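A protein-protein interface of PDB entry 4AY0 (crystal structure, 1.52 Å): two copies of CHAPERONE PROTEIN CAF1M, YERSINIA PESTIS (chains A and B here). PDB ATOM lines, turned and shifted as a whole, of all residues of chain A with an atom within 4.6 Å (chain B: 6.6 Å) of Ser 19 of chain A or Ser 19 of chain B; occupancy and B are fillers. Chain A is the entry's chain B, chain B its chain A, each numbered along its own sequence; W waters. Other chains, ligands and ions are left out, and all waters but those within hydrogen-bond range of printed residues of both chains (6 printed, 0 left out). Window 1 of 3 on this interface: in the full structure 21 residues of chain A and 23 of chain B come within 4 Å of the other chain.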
ATOM      1  N   ILE A  16     -31.248   3.990  13.163  1.00  0.00           N
ATOM      2  CA  ILE A  16     -31.702   4.845  14.255  1.00  0.00           C
ATOM      3  C   ILE A  16     -30.570   5.799  14.618  1.00  0.00           C
ATOM      4  O   ILE A  16     -29.445   5.371  14.897  1.00  0.00           O
ATOM      5  CB  ILE A  16     -32.079   4.025  15.508  1.00  0.00           C
ATOM      6  CG1 ILE A  16     -33.016   2.867  15.164  1.00  0.00           C
ATOM      7  CG2 ILE A  16     -32.712   4.922  16.566  1.00  0.00           C
ATOM      8  CD1 ILE A  16     -33.218   1.883  16.334  1.00  0.00           C
ATOM      9  N   GLY A  17     -30.865   7.095  14.626  1.00  0.00           N
ATOM     10  CA  GLY A  17     -29.847   8.089  14.917  1.00  0.00           C
ATOM     11  C   GLY A  17     -28.920   8.295  13.737  1.00  0.00           C
ATOM     12  O   GLY A  17     -29.116   7.709  12.670  1.00  0.00           O
ATOM     13  N   GLU A  18     -27.920   9.143  13.918  1.00  0.00           N
ATOM     14  CA  GLU A  18     -26.965   9.390  12.852  1.00  0.00           C
ATOM     15  C   GLU A  18     -25.592   9.607  13.451  1.00  0.00           C
ATOM     16  O   GLU A  18     -25.297  10.679  13.977  1.00  0.00           O
ATOM     17  CB  GLU A  18     -27.386  10.603  12.030  1.00  0.00           C
ATOM     18  CG  GLU A  18     -26.576  10.769  10.762  1.00  0.00           C
ATOM     19  CD  GLU A  18     -26.857  12.087  10.070  1.00  0.00           C
ATOM     20  OE1 GLU A  18     -27.999  12.285   9.600  1.00  0.00           O
ATOM     21  OE2 GLU A  18     -25.933  12.926  10.008  1.00  0.00           O
ATOM     22  N   SER A  19     -24.757   8.583  13.394  1.00  0.00           N
ATOM     23  CA  SER A  19     -23.425   8.685  13.967  1.00  0.00           C
ATOM     24  C   SER A  19     -22.537   9.672  13.212  1.00  0.00           C
ATOM     25  O   SER A  19     -22.709   9.913  12.011  1.00  0.00           O
ATOM     26  CB  SER A  19     -22.774   7.307  14.036  1.00  0.00           C
ATOM     27  OG  SER A  19     -23.524   6.458  14.891  1.00  0.00           O
ATOM     28  N   ARG A  20     -21.595  10.250  13.950  1.00  0.00           N
ATOM     29  CA  ARG A  20     -20.561  11.111  13.392  1.00  0.00           C
ATOM     30  C   ARG A  20     -19.295  10.813  14.190  1.00  0.00           C
ATOM     31  O   ARG A  20     -19.352  10.289  15.313  1.00  0.00           O
ATOM     32  CB  ARG A  20     -20.920  12.596  13.506  1.00  0.00           C
ATOM     33  CG  ARG A  20     -21.434  13.023  14.887  1.00  0.00           C
ATOM     34  CD  ARG A  20     -22.976  13.032  14.974  1.00  0.00           C
ATOM     35  NE  ARG A  20     -23.472  14.169  14.207  1.00  0.00           N
ATOM     36  CZ  ARG A  20     -24.076  14.097  13.025  1.00  0.00           C
ATOM     37  NH1 ARG A  20     -24.368  12.928  12.478  1.00  0.00           N
ATOM     38  NH2 ARG A  20     -24.424  15.212  12.403  1.00  0.00           N
ATOM     39  N   ILE A 121     -19.999   8.769   6.602  1.00  0.00           N
ATOM     40  CA  ILE A 121     -20.200   9.333   7.933  1.00  0.00           C
ATOM     41  C   ILE A 121     -19.339  10.589   8.065  1.00  0.00           C
ATOM     42  O   ILE A 121     -18.215  10.633   7.557  1.00  0.00           O
ATOM     43  CB  ILE A 121     -19.830   8.296   9.028  1.00  0.00           C
ATOM     44  CG1 ILE A 121     -20.036   8.869  10.426  1.00  0.00           C
ATOM     45  CG2 ILE A 121     -18.394   7.815   8.873  1.00  0.00           C
ATOM     46  CD1 ILE A 121     -19.869   7.844  11.519  1.00  0.00           C
ATOM     47  N   ILE B  16     -21.141   1.981  10.802  1.00  0.00           N
ATOM     48  CA  ILE B  16     -19.955   2.639  11.328  1.00  0.00           C
ATOM     49  C   ILE B  16     -20.297   3.217  12.703  1.00  0.00           C
ATOM     50  O   ILE B  16     -21.255   3.988  12.841  1.00  0.00           O
ATOM     51  CB  ILE B  16     -19.480   3.766  10.388  1.00  0.00           C
ATOM     52  CG1 ILE B  16     -19.275   3.236   8.963  1.00  0.00           C
ATOM     53  CG2 ILE B  16     -18.197   4.388  10.907  1.00  0.00           C
ATOM     54  CD1 ILE B  16     -19.092   4.323   7.921  1.00  0.00           C
ATOM     55  N   GLY B  17     -19.522   2.843  13.721  1.00  0.00           N
ATOM     56  CA  GLY B  17     -19.807   3.279  15.083  1.00  0.00           C
ATOM     57  C   GLY B  17     -21.060   2.635  15.638  1.00  0.00           C
ATOM     58  O   GLY B  17     -21.620   1.712  15.043  1.00  0.00           O
ATOM     59  N   GLU B  18     -21.515   3.123  16.783  1.00  0.00           N
ATOM     60  CA  GLU B  18     -22.690   2.544  17.408  1.00  0.00           C
ATOM     61  C   GLU B  18     -23.430   3.601  18.200  1.00  0.00           C
ATOM     62  O   GLU B  18     -23.005   3.981  19.292  1.00  0.00           O
ATOM     63  CB  GLU B  18     -22.287   1.385  18.322  1.00  0.00           C
ATOM     64  CG  GLU B  18     -23.474   0.697  18.955  1.00  0.00           C
ATOM     65  CD  GLU B  18     -23.064  -0.359  19.954  1.00  0.00           C
ATOM     66  OE1 GLU B  18     -22.420  -1.351  19.554  1.00  0.00           O
ATOM     67  OE2 GLU B  18     -23.394  -0.197  21.140  1.00  0.00           O
ATOM     68  N   SER B  19     -24.528   4.097  17.642  1.00  0.00           N
ATOM     69  CA  SER B  19     -25.290   5.130  18.319  1.00  0.00           C
ATOM     70  C   SER B  19     -25.925   4.616  19.610  1.00  0.00           C
ATOM     71  O   SER B  19     -26.244   3.424  19.741  1.00  0.00           O
ATOM     72  CB  SER B  19     -26.359   5.700  17.387  1.00  0.00           C
ATOM     73  OG  SER B  19     -25.741   6.309  16.270  1.00  0.00           O
ATOM     74  N   ARG B  20     -26.064   5.538  20.560  1.00  0.00           N
ATOM     75  CA  ARG B  20     -26.834   5.318  21.781  1.00  0.00           C
ATOM     76  C   ARG B  20     -27.598   6.605  22.053  1.00  0.00           C
ATOM     77  O   ARG B  20     -27.251   7.658  21.520  1.00  0.00           O
ATOM     78  CB  ARG B  20     -25.908   4.997  22.965  1.00  0.00           C
ATOM     79  CG  ARG B  20     -24.702   5.953  23.127  1.00  0.00           C
ATOM     80  CD  ARG B  20     -23.411   5.416  22.480  1.00  0.00           C
ATOM     81  NE  ARG B  20     -22.910   4.312  23.299  1.00  0.00           N
ATOM     82  CZ  ARG B  20     -22.984   3.026  22.974  1.00  0.00           C
ATOM     83  NH1 ARG B  20     -23.451   2.636  21.801  1.00  0.00           N
ATOM     84  NH2 ARG B  20     -22.554   2.121  23.823  1.00  0.00           N
ATOM     85  N   ILE B  21     -28.626   6.518  22.889  1.00  0.00           N
ATOM     86  CA  ILE B  21     -29.437   7.670  23.242  1.00  0.00           C
ATOM     87  C   ILE B  21     -29.217   7.977  24.711  1.00  0.00           C
ATOM     88  O   ILE B  21     -29.410   7.103  25.556  1.00  0.00           O
ATOM     89  CB  ILE B  21     -30.940   7.377  22.994  1.00  0.00           C
ATOM     90  CG1 ILE B  21     -31.151   7.015  21.516  1.00  0.00           C
ATOM     91  CG2 ILE B  21     -31.806   8.577  23.365  1.00  0.00           C
ATOM     92  CD1 ILE B  21     -32.530   6.475  21.194  1.00  0.00           C
ATOM     93  N   CYS B 120     -32.109  -2.427  17.497  1.00  0.00           N
ATOM     94  CA  CYS B 120     -32.206  -1.966  18.878  1.00  0.00           C
ATOM     95  C   CYS B 120     -31.050  -1.028  19.225  1.00  0.00           C
ATOM     96  O   CYS B 120     -29.905  -1.246  18.808  1.00  0.00           O
ATOM     97  CB  CYS B 120     -32.227  -3.155  19.844  1.00  0.00           C
ATOM     98  SG  CYS B 120     -33.677  -4.242  19.692  1.00  0.00           S
ATOM     99  N   ILE B 121     -31.360   0.014  19.988  1.00  0.00           N
ATOM    100  CA  ILE B 121     -30.370   0.999  20.412  1.00  0.00           C
ATOM    101  C   ILE B 121     -30.495   1.221  21.918  1.00  0.00           C
ATOM    102  O   ILE B 121     -31.600   1.198  22.460  1.00  0.00           O
ATOM    103  CB  ILE B 121     -30.563   2.329  19.638  1.00  0.00           C
ATOM    104  CG1 ILE B 121     -29.471   3.343  19.985  1.00  0.00           C
ATOM    105  CG2 ILE B 121     -31.954   2.917  19.877  1.00  0.00           C
ATOM    106  CD1 ILE B 121     -29.526   4.594  19.128  1.00  0.00           C
ATOM    107  N   LYS B 122     -29.364   1.406  22.599  1.00  0.00           N
ATOM    108  CA  LYS B 122     -29.372   1.641  24.044  1.00  0.00           C
ATOM    109  C   LYS B 122     -29.957   2.996  24.385  1.00  0.00           C
ATOM    110  O   LYS B 122     -29.649   3.993  23.727  1.00  0.00           O
ATOM    111  CB  LYS B 122     -27.955   1.534  24.620  1.00  0.00           C
ATOM    112  CG  LYS B 122     -27.417   0.108  24.602  1.00  0.00           C
ATOM    113  CD  LYS B 122     -25.991   0.025  25.127  1.00  0.00           C
ATOM    114  CE  LYS B 122     -25.548  -1.449  25.196  1.00  0.00           C
ATOM    115  NZ  LYS B 122     -24.086  -1.600  25.256  1.00  0.00           N
ATOM    116  N   ASP B 204     -19.902   8.417  24.601  1.00  0.00           N
ATOM    117  CA  ASP B 204     -21.283   8.867  24.389  1.00  0.00           C
ATOM    118  C   ASP B 204     -21.595   9.100  22.910  1.00  0.00           C
ATOM    119  O   ASP B 204     -22.758   9.022  22.489  1.00  0.00           O
ATOM    120  CB  ASP B 204     -21.544  10.164  25.156  1.00  0.00           C
ATOM    121  CG  ASP B 204     -21.774   9.955  26.646  1.00  0.00           C
ATOM    122  OD1 ASP B 204     -21.981   8.813  27.107  1.00  0.00           O
ATOM    123  OD2 ASP B 204     -21.752  10.979  27.352  1.00  0.00           O
ATOM    124  N   GLN B 205     -20.562   9.394  22.122  1.00  0.00           N
ATOM    125  CA  GLN B 205     -20.738   9.692  20.704  1.00  0.00           C
ATOM    126  C   GLN B 205     -20.744   8.439  19.836  1.00  0.00           C
ATOM    127  O   GLN B 205     -20.831   8.522  18.611  1.00  0.00           O
ATOM    128  CB  GLN B 205     -19.667  10.679  20.225  1.00  0.00           C
ATOM    129  CG  GLN B 205     -19.745  12.062  20.885  1.00  0.00           C
ATOM    130  CD  GLN B 205     -19.333  12.056  22.345  1.00  0.00           C
ATOM    131  OE1 GLN B 205     -20.062  12.553  23.205  1.00  0.00           O
ATOM    132  NE2 GLN B 205     -18.173  11.482  22.633  1.00  0.00           N
ATOM    133  N   GLY B 206     -20.658   7.272  20.468  1.00  0.00           N
ATOM    134  CA  GLY B 206     -20.723   6.028  19.724  1.00  0.00           C
ATOM    135  C   GLY B 206     -19.394   5.570  19.151  1.00  0.00           C
ATOM    136  O   GLY B 206     -19.341   4.612  18.375  1.00  0.00           O
HETATM  137  O   HOH W   1     -21.658   6.180  16.714  1.00  0.00           O
HETATM  138  O   HOH W   2     -23.642   4.104  13.287  1.00  0.00           O
HETATM  139  O   HOH W   3     -23.951   8.074  17.364  1.00  0.00           O
HETATM  140  O   HOH W   4     -26.958   5.308  14.152  1.00  0.00           O
HETATM  141  O   HOH W   5     -18.363   8.470  17.034  1.00  0.00           O
HETATM  142  O   HOH W   6     -22.291  10.341  17.131  1.00  0.00           O
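The side-chain hydroxyl (OG) of Ser 19 of chain B lies within hydrogen-bond range of the side-chain hydroxyl (OG) of Ser 19 of chain A, 2.6 Å away.
Ser 19 of chain B touches Ile 16 of chain A. Ile 16 of chain A touches Ile 121 of chain B. Ile 16 of chain B touches Ser 19 of chain A. Ile 16 of chain B touches Ile 121 of chain A.
Of the printed residues of chain B, Ser 19 of chain A touches Ile 16 (3.8 Å) and Ser 19 (2.6 Å). Printed residues of chain A within 4 Å of Ser 19 of chain B: Ile 16 and Ser 19. Printed residues of chain A within 4 Å of Ile 16 of chain B: Ser 19 (3.8 Å) and Ile 121 (3.7 Å). Of the printed residues of chain A, Ile 121 of chain B touches Ile 16 (3.9 Å). Of the printed residues of chain B, Ile 16 of chain A touches Ser 19 (3.98 Å) and Ile 121 (3.9 Å). Of the printed residues of chain B, Ile 121 of chain A touches Ile 16 (3.7 Å). Glu 18 of chain B touches none of the printed residues of chain A. Arg 20 of chain A touches none of the printed residues of chain B. The nearest printed residue of chain A that does not touch Ser 19 of chain B is Glu 18 of chain A (4.3 Å).
Printed residues of chain A that touch a printed residue of chain B: Ile 16, Ser 19 and Ile 121. Along chain A the printed residues that touch a printed residue of chain B span positions 16 to 121. Of the 12 printed residues of chain B, 3 touch a printed residue of chain A. Among the printed residues, 5 pairs touch across the chains. Among the printed residues, no Asp or Glu carboxylate lies within 4 Å of a Lys or Arg side-chain nitrogen of the other chain.
Ile 16 of chain A touches Ser 19 of chain B, and with the chains exchanged Ser 19 of chain A touches Ile 16 of chain B. Ile 16 of chain A touches Ile 121 of chain B, and with the chains exchanged Ile 121 of chain A touches Ile 16 of chain B. Ser 19 of chain A touches its own counterpart, Ser 19 of chain B. Positions printed for both chains: 16, 17, 18, 19, 20 and 121. Of the 5 pairs that touch across the chains among the printed residues, 5 have their exchanged pair printed and touching as well.
Water W2 lies within hydrogen-bond range of the backbone carbonyl oxygen of Ile 16 of chain B (2.4 Å) and the side-chain hydroxyl of Ser 19 of chain A (2.9 Å). Water W4 bridges the backbone carbonyl oxygen (O) of Ile 16 of chain A (2.6 Å) and the side-chain hydroxyl (OG) of Ser 19 of chain B (2.6 Å). Water W1 lies within hydrogen-bond range of the side-chain hydroxyl (OG) of Ser 19 of chain A (2.6 Å), the backbone NH (N) of Glu 18 of chain B (3.1 Å), the backbone carbonyl oxygen (O) of Gln 205 of chain B (3.1 Å) and the backbone carbonyl oxygen (O) of Gly 206 of chain B (3.3 Å). Water W5 bridges O of Arg 20 of chain A (2.7 Å) and O of Gln 205 of chain B (2.9 Å). Water W3 lies within hydrogen-bond range of the side-chain hydroxyl (OG) of Ser 19 of chain B, the side-chain hydroxyl (OG) of Ser 19 of chain A and the backbone carbonyl oxygen (O) of Gln 205 of chain B. Water W6 bridges O of Gln 205 of chain B and N of Arg 20 of chain A.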
